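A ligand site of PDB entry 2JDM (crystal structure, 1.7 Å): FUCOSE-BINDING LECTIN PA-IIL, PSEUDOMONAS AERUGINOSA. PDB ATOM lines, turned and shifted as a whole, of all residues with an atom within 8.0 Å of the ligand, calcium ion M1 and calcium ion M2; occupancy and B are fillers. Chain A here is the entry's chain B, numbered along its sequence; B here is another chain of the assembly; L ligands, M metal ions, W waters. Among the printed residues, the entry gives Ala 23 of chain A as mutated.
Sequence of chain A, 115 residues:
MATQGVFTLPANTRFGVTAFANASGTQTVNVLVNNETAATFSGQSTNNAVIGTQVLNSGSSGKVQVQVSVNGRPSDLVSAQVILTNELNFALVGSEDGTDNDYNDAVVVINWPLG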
ATOM      1  N   ALA A  21      15.786  11.740  24.099  1.00  0.00           N
ATOM      2  CA  ALA A  21      14.549  12.448  24.475  1.00  0.00           C
ATOM      3  C   ALA A  21      13.338  11.518  24.506  1.00  0.00           C
ATOM      4  O   ALA A  21      13.161  10.666  23.599  1.00  0.00           O
ATOM      5  CB  ALA A  21      14.287  13.618  23.531  1.00  0.00           C
ATOM      6  N   ASN A  22      12.474  11.735  25.491  1.00  0.00           N
ATOM      7  CA  ASN A  22      11.260  10.945  25.703  1.00  0.00           C
ATOM      8  C   ASN A  22      10.214  11.803  26.420  1.00  0.00           C
ATOM      9  O   ASN A  22       9.911  11.577  27.585  1.00  0.00           O
ATOM     10  CB  ASN A  22      11.510   9.700  26.530  1.00  0.00           C
ATOM     11  CG  ASN A  22      12.341   8.694  25.807  1.00  0.00           C
ATOM     12  OD1 ASN A  22      11.862   8.004  24.916  1.00  0.00           O
ATOM     13  ND2 ASN A  22      13.598   8.582  26.189  1.00  0.00           N
ATOM     14  N   ALA A  23       9.643  12.763  25.693  1.00  0.00           N
ATOM     15  CA  ALA A  23       8.663  13.692  26.261  1.00  0.00           C
ATOM     16  C   ALA A  23       7.931  14.459  25.181  1.00  0.00           C
ATOM     17  O   ALA A  23       8.369  14.498  24.027  1.00  0.00           O
ATOM     18  CB  ALA A  23       9.358  14.662  27.231  1.00  0.00           C
ATOM     19  N   SER A  24       6.796  15.077  25.521  1.00  0.00           N
ATOM     20  CA  SER A  24       6.084  15.871  24.521  1.00  0.00           C
ATOM     21  C   SER A  24       6.792  17.182  24.190  1.00  0.00           C
ATOM     22  O   SER A  24       6.650  17.702  23.090  1.00  0.00           O
ATOM     23  CB  SER A  24       4.641  16.147  24.955  1.00  0.00           C
ATOM     24  OG  SER A  24       4.609  16.912  26.127  1.00  0.00           O
ATOM     25  N   GLY A  25       7.543  17.725  25.146  1.00  0.00           N
ATOM     26  CA  GLY A  25       8.174  19.038  24.983  1.00  0.00           C
ATOM     27  C   GLY A  25       9.633  18.970  24.537  1.00  0.00           C
ATOM     28  O   GLY A  25      10.340  17.983  24.788  1.00  0.00           O
ATOM     29  N   GLN A  27      13.393  19.174  24.585  1.00  0.00           N
ATOM     30  CA  GLN A  27      14.419  19.085  25.622  1.00  0.00           C
ATOM     31  C   GLN A  27      15.622  19.902  25.205  1.00  0.00           C
ATOM     32  O   GLN A  27      16.046  19.854  24.052  1.00  0.00           O
ATOM     33  CB  GLN A  27      14.840  17.627  25.853  1.00  0.00           C
ATOM     34  CG  GLN A  27      13.677  16.688  26.146  1.00  0.00           C
ATOM     35  CD  GLN A  27      12.979  16.973  27.466  1.00  0.00           C
ATOM     36  OE1 GLN A  27      13.613  17.017  28.514  1.00  0.00           O
ATOM     37  NE2 GLN A  27      11.655  17.140  27.417  1.00  0.00           N
ATOM     38  N   GLN A  44      12.779  17.250  20.321  1.00  0.00           N
ATOM     39  CA  GLN A  44      11.619  16.572  20.884  1.00  0.00           C
ATOM     40  C   GLN A  44      11.452  15.171  20.298  1.00  0.00           C
ATOM     41  O   GLN A  44      11.523  14.978  19.091  1.00  0.00           O
ATOM     42  CB  GLN A  44      10.343  17.386  20.614  1.00  0.00           C
ATOM     43  CG  GLN A  44       9.051  16.838  21.312  1.00  0.00           C
ATOM     44  CD  GLN A  44       8.337  15.696  20.557  1.00  0.00           C
ATOM     45  OE1 GLN A  44       8.209  15.734  19.335  1.00  0.00           O
ATOM     46  NE2 GLN A  44       7.849  14.712  21.293  1.00  0.00           N
ATOM     47  N   SER A  45      11.185  14.211  21.173  1.00  0.00           N
ATOM     48  CA  SER A  45      10.920  12.834  20.762  1.00  0.00           C
ATOM     49  C   SER A  45      10.219  12.095  21.886  1.00  0.00           C
ATOM     50  O   SER A  45      10.495  12.326  23.055  1.00  0.00           O
ATOM     51  CB  SER A  45      12.232  12.107  20.408  1.00  0.00           C
ATOM     52  OG  SER A  45      11.982  10.750  20.036  1.00  0.00           O
ATOM     53  N   THR A  46       9.324  11.185  21.518  1.00  0.00           N
ATOM     54  CA  THR A  46       8.757  10.236  22.497  1.00  0.00           C
ATOM     55  C   THR A  46       9.226   8.818  22.167  1.00  0.00           C
ATOM     56  O   THR A  46       8.649   7.841  22.646  1.00  0.00           O
ATOM     57  CB  THR A  46       7.220  10.314  22.547  1.00  0.00           C
ATOM     58  OG1 THR A  46       6.697  10.253  21.213  1.00  0.00           O
ATOM     59  CG2 THR A  46       6.777  11.580  23.200  1.00  0.00           C
ATOM     60  N   VAL A  70      13.416  22.627  29.791  1.00  0.00           N
ATOM     61  CA  VAL A  70      12.356  22.578  28.808  1.00  0.00           C
ATOM     62  C   VAL A  70      11.729  23.984  28.743  1.00  0.00           C
ATOM     63  O   VAL A  70      11.142  24.453  29.724  1.00  0.00           O
ATOM     64  CB  VAL A  70      11.332  21.463  29.145  1.00  0.00           C
ATOM     65  CG1 VAL A  70      10.185  21.476  28.150  1.00  0.00           C
ATOM     66  CG2 VAL A  70      12.027  20.095  29.138  1.00  0.00           C
ATOM     67  N   SER A  95      16.221  12.869  33.855  1.00  0.00           N
ATOM     68  CA  SER A  95      15.616  14.167  34.171  1.00  0.00           C
ATOM     69  C   SER A  95      14.111  14.128  34.041  1.00  0.00           C
ATOM     70  O   SER A  95      13.567  13.380  33.232  1.00  0.00           O
ATOM     71  CB  SER A  95      16.174  15.269  33.271  1.00  0.00           C
ATOM     72  OG  SER A  95      15.918  15.045  31.889  1.00  0.00           O
ATOM     73  N   GLU A  96      13.428  14.945  34.859  1.00  0.00           N
ATOM     74  CA  GLU A  96      11.958  14.963  34.852  1.00  0.00           C
ATOM     75  C   GLU A  96      11.452  16.398  34.658  1.00  0.00           C
ATOM     76  O   GLU A  96      11.809  17.304  35.431  1.00  0.00           O
ATOM     77  CB  GLU A  96      11.449  14.409  36.203  1.00  0.00           C
ATOM     78  CG  GLU A  96       9.941  14.366  36.398  1.00  0.00           C
ATOM     79  CD  GLU A  96       9.222  13.707  35.261  1.00  0.00           C
ATOM     80  OE1 GLU A  96       9.558  12.536  34.889  1.00  0.00           O
ATOM     81  OE2 GLU A  96       8.309  14.352  34.694  1.00  0.00           O
ATOM     82  N   ASP A  97      10.604  16.590  33.639  1.00  0.00           N
ATOM     83  CA  ASP A  97      10.130  17.931  33.267  1.00  0.00           C
ATOM     84  C   ASP A  97       8.715  18.194  33.749  1.00  0.00           C
ATOM     85  O   ASP A  97       8.176  19.292  33.524  1.00  0.00           O
ATOM     86  CB  ASP A  97      10.250  18.156  31.744  1.00  0.00           C
ATOM     87  CG  ASP A  97       9.320  17.253  30.932  1.00  0.00           C
ATOM     88  OD1 ASP A  97       8.243  16.836  31.422  1.00  0.00           O
ATOM     89  OD2 ASP A  97       9.641  16.989  29.738  1.00  0.00           O
ATOM     90  N   GLY A  98       8.127  17.200  34.420  1.00  0.00           N
ATOM     91  CA  GLY A  98       6.695  17.170  34.661  1.00  0.00           C
ATOM     92  C   GLY A  98       6.341  16.509  35.978  1.00  0.00           C
ATOM     93  O   GLY A  98       7.050  16.718  36.984  1.00  0.00           O
ATOM     94  N   THR A  99       5.253  15.740  35.954  1.00  0.00           N
ATOM     95  CA  THR A  99       4.667  15.160  37.175  1.00  0.00           C
ATOM     96  C   THR A  99       4.623  13.640  37.247  1.00  0.00           C
ATOM     97  O   THR A  99       4.347  13.087  38.314  1.00  0.00           O
ATOM     98  CB  THR A  99       3.218  15.686  37.405  1.00  0.00           C
ATOM     99  OG1 THR A  99       2.371  15.261  36.328  1.00  0.00           O
ATOM    100  CG2 THR A  99       3.202  17.202  37.543  1.00  0.00           C
ATOM    101  N   ASP A 100       4.882  12.946  36.134  1.00  0.00           N
ATOM    102  CA  ASP A 100       4.721  11.483  36.120  1.00  0.00           C
ATOM    103  C   ASP A 100       5.933  10.732  36.677  1.00  0.00           C
ATOM    104  O   ASP A 100       5.841   9.534  36.974  1.00  0.00           O
ATOM    105  CB  ASP A 100       4.346  11.000  34.707  1.00  0.00           C
ATOM    106  CG  ASP A 100       5.481  11.122  33.720  1.00  0.00           C
ATOM    107  OD1 ASP A 100       6.441  11.885  33.979  1.00  0.00           O
ATOM    108  OD2 ASP A 100       5.414  10.453  32.677  1.00  0.00           O
ATOM    109  N   ASN A 101       7.045  11.437  36.839  1.00  0.00           N
ATOM    110  CA  ASN A 101       8.277  10.915  37.424  1.00  0.00           C
ATOM    111  C   ASN A 101       8.841   9.695  36.719  1.00  0.00           C
ATOM    112  O   ASN A 101       9.368   8.771  37.366  1.00  0.00           O
ATOM    113  CB  ASN A 101       8.128  10.674  38.953  1.00  0.00           C
ATOM    114  CG  ASN A 101       7.942  11.984  39.716  1.00  0.00           C
ATOM    115  OD1 ASN A 101       8.297  13.048  39.217  1.00  0.00           O
ATOM    116  ND2 ASN A 101       7.361  11.896  40.911  1.00  0.00           N
ATOM    117  N   ASP A 102       8.750   9.700  35.388  1.00  0.00           N
ATOM    118  CA  ASP A 102       9.449   8.643  34.640  1.00  0.00           C
ATOM    119  C   ASP A 102      10.950   8.946  34.514  1.00  0.00           C
ATOM    120  O   ASP A 102      11.755   8.036  34.285  1.00  0.00           O
ATOM    121  CB  ASP A 102       8.777   8.234  33.313  1.00  0.00           C
ATOM    122  CG  ASP A 102       8.686   9.377  32.278  1.00  0.00           C
ATOM    123  OD1 ASP A 102       9.141  10.510  32.570  1.00  0.00           O
ATOM    124  OD2 ASP A 102       8.157   9.125  31.168  1.00  0.00           O
ATOM    125  N   TYR A 103      11.332  10.217  34.709  1.00  0.00           N
ATOM    126  CA  TYR A 103      12.744  10.625  34.716  1.00  0.00           C
ATOM    127  C   TYR A 103      13.504  10.265  33.442  1.00  0.00           C
ATOM    128  O   TYR A 103      14.715  10.071  33.468  1.00  0.00           O
ATOM    129  CB  TYR A 103      13.485  10.167  36.000  1.00  0.00           C
ATOM    130  CG  TYR A 103      13.208  11.110  37.163  1.00  0.00           C
ATOM    131  CD1 TYR A 103      12.046  10.959  37.956  1.00  0.00           C
ATOM    132  CD2 TYR A 103      14.056  12.193  37.418  1.00  0.00           C
ATOM    133  CE1 TYR A 103      11.784  11.865  39.000  1.00  0.00           C
ATOM    134  CE2 TYR A 103      13.811  13.074  38.427  1.00  0.00           C
ATOM    135  CZ  TYR A 103      12.671  12.904  39.227  1.00  0.00           C
ATOM    136  OH  TYR A 103      12.434  13.814  40.231  1.00  0.00           O
ATOM    137  N   ASN A 104      12.781  10.189  32.324  1.00  0.00           N
ATOM    138  CA  ASN A 104      13.372   9.787  31.051  1.00  0.00           C
ATOM    139  C   ASN A 104      13.213  10.890  30.023  1.00  0.00           C
ATOM    140  O   ASN A 104      13.521  10.684  28.837  1.00  0.00           O
ATOM    141  CB  ASN A 104      12.734   8.478  30.536  1.00  0.00           C
ATOM    142  CG  ASN A 104      11.335   8.675  29.979  1.00  0.00           C
ATOM    143  OD1 ASN A 104      10.778   9.777  30.052  1.00  0.00           O
ATOM    144  ND2 ASN A 104      10.754   7.614  29.411  1.00  0.00           N
ATOM    145  N   ASP A 105      12.705  12.047  30.456  1.00  0.00           N
ATOM    146  CA  ASP A 105      12.349  13.117  29.518  1.00  0.00           C
ATOM    147  C   ASP A 105      13.550  13.564  28.711  1.00  0.00           C
ATOM    148  O   ASP A 105      13.477  13.670  27.478  1.00  0.00           O
ATOM    149  CB  ASP A 105      11.662  14.281  30.255  1.00  0.00           C
ATOM    150  CG  ASP A 105      10.439  13.801  31.042  1.00  0.00           C
ATOM    151  OD1 ASP A 105       9.748  12.891  30.545  1.00  0.00           O
ATOM    152  OD2 ASP A 105      10.173  14.287  32.151  1.00  0.00           O
ATOM    153  N   ALA A 106      14.668  13.800  29.405  1.00  0.00           N
ATOM    154  CA  ALA A 106      15.977  13.712  28.758  1.00  0.00           C
ATOM    155  C   ALA A 106      16.862  12.752  29.551  1.00  0.00           C
ATOM    156  O   ALA A 106      16.878  12.787  30.799  1.00  0.00           O
ATOM    157  CB  ALA A 106      16.622  15.096  28.583  1.00  0.00           C
ATOM    158  N   PRO B 113      11.995   2.929  30.862  1.00  0.00           N
ATOM    159  CA  PRO B 113      11.010   2.946  29.801  1.00  0.00           C
ATOM    160  C   PRO B 113      11.206   4.130  28.880  1.00  0.00           C
ATOM    161  O   PRO B 113      11.963   5.050  29.207  1.00  0.00           O
ATOM    162  CB  PRO B 113       9.701   3.114  30.558  1.00  0.00           C
ATOM    163  CG  PRO B 113      10.061   3.954  31.673  1.00  0.00           C
ATOM    164  CD  PRO B 113      11.396   3.415  32.124  1.00  0.00           C
ATOM    165  N   LEU B 114      10.545   4.104  27.724  1.00  0.00           N
ATOM    166  CA  LEU B 114      10.601   5.224  26.795  1.00  0.00           C
ATOM    167  C   LEU B 114       9.304   6.035  26.868  1.00  0.00           C
ATOM    168  O   LEU B 114       8.428   5.745  27.679  1.00  0.00           O
ATOM    169  CB  LEU B 114      10.832   4.727  25.368  1.00  0.00           C
ATOM    170  CG  LEU B 114      12.034   3.808  25.144  1.00  0.00           C
ATOM    171  CD1 LEU B 114      12.119   3.510  23.641  1.00  0.00           C
ATOM    172  CD2 LEU B 114      13.330   4.396  25.688  1.00  0.00           C
ATOM    173  N   GLY B 115       9.185   7.041  26.001  1.00  0.00           N
ATOM    174  CA  GLY B 115       7.973   7.847  25.889  1.00  0.00           C
ATOM    175  C   GLY B 115       7.776   8.934  26.904  1.00  0.00           C
ATOM    176  O   GLY B 115       8.457   9.002  27.935  1.00  0.00           O
ATOM    177  OXT GLY B 115       6.881   9.767  26.688  1.00  0.00           O
HETATM  178  C1  LIG L   1       5.771  14.909  29.357  1.00  0.00           C
HETATM  179  C2  LIG L   1       6.690  14.009  30.201  1.00  0.00           C
HETATM  180  C3  LIG L   1       6.063  12.624  30.360  1.00  0.00           C
HETATM  181  C4  LIG L   1       5.651  12.053  29.002  1.00  0.00           C
HETATM  182  C5  LIG L   1       4.809  13.040  28.170  1.00  0.00           C
HETATM  183  C6  LIG L   1       4.474  12.480  26.793  1.00  0.00           C
HETATM  184  O1  LIG L   1       4.544  15.120  30.068  1.00  0.00           O
HETATM  185  O2  LIG L   1       7.019  14.539  31.519  1.00  0.00           O
HETATM  186  O3  LIG L   1       7.032  11.724  30.915  1.00  0.00           O
HETATM  187  O4  LIG L   1       6.844  11.716  28.279  1.00  0.00           O
HETATM  188  O5  LIG L   1       5.505  14.297  28.080  1.00  0.00           O
HETATM  189  C7  LIG L   1       3.724  16.198  29.566  1.00  0.00           C
HETATM  190 CA    CA M   1       8.775  10.813  29.608  1.00  0.00          CA
HETATM  191 CA    CA M   2       8.331  12.765  32.732  1.00  0.00          CA
HETATM  192  O   HOH W   1       2.017  15.717  26.579  1.00  0.00           O
HETATM  193  O   HOH W   2       3.764  18.001  32.258  1.00  0.00           O
HETATM  194  O   HOH W   3       4.533  14.542  33.239  1.00  0.00           O
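OD1 of Asp 97 lies close to O2 of the ligand, 2.6 Å away.
OG of Ser 24 is in hydrogen-bond range of O5 of the ligand (3.4 Å).
An oxygen (O5) of the ligand is in hydrogen-bond range of the backbone NH of Ser 24 (3.0 Å).
ND2 of Asn 104 sits close to O of Leu 114 of chain B (3.5 Å).
NE2 of Gln 27 lies within hydrogen-bond range of OD2 of Asp 97 (3.1 Å).
The backbone carbonyl oxygen of Ser 95 lies within hydrogen-bond range of the backbone NH of Asn 104 (3.4 Å).
The backbone NH (N) of Asp 105 lies within hydrogen-bond range of the backbone carbonyl oxygen (O) of Ser 95 (3.2 Å).
The backbone carbonyl oxygen (O) of Pro 113 of chain B is in hydrogen-bond range of the side-chain amide nitrogen (ND2) of Asn 104, at 2.8 Å.
The backbone NH of Ala 23 is in hydrogen-bond range of the backbone carbonyl oxygen of Ser 45, at 2.8 Å.
The side-chain carboxylate (OD2) of Asp 105 sits close to the backbone NH (N) of Asp 97 (2.8 Å).
The backbone NH of Gly 115 of chain B lies close to the backbone carbonyl oxygen of Thr 46 (3.5 Å).
Ala 23 touches the ligand.
Hydrophobic or aromatic side chains within 4 Å of the ligand: Ala 23.
Of the 25 residues printed, 9 come within 4 Å of the ligand.
Of the 25 residues printed, 5 come within 4 Å of calcium ion M1.
The nearest printed residue that does not touch calcium ion M1 is Ala 23 (4.4 Å).
Calcium ion M1 is bound by the side-chain amide oxygen (OD1) of Asn 104 (2.3 Å), an oxygen (O3) of the ligand (2.4 Å), the side-chain carboxylate (OD2) of Asp 102 (2.4 Å), the backbone carbonyl oxygen (O) of Asn 22 (2.4 Å), the side-chain carboxylate (OD1) of Asp 105 (2.5 Å), the chain-end carboxylate (O) of Gly 115 of chain B (2.5 Å) and an oxygen (O4) of the ligand (2.5 Å).
Slightly farther from calcium ion M1 lies OD1 of Asp 102 (3.0 Å).
Calcium ion M2 is bound by OD1 of Asp 102 (2.4 Å), OD1 of Asp 100 (2.4 Å), OD2 of Asp 105 (2.5 Å), O3 of the ligand (2.5 Å), OE1 of Glu 96 (2.5 Å), O2 of the ligand (2.5 Å), OE2 of Glu 96 (2.5 Å) and OD1 of Asp 105 (2.6 Å).
Calcium ion M2 has eight donor atoms within binding distance.
Water W3 lies within hydrogen-bond range of the backbone NH (N) of Thr 99 (3.1 Å), an oxygen (O1) of the ligand (3.2 Å) and the backbone NH (N) of Asp 100 (3.3 Å).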
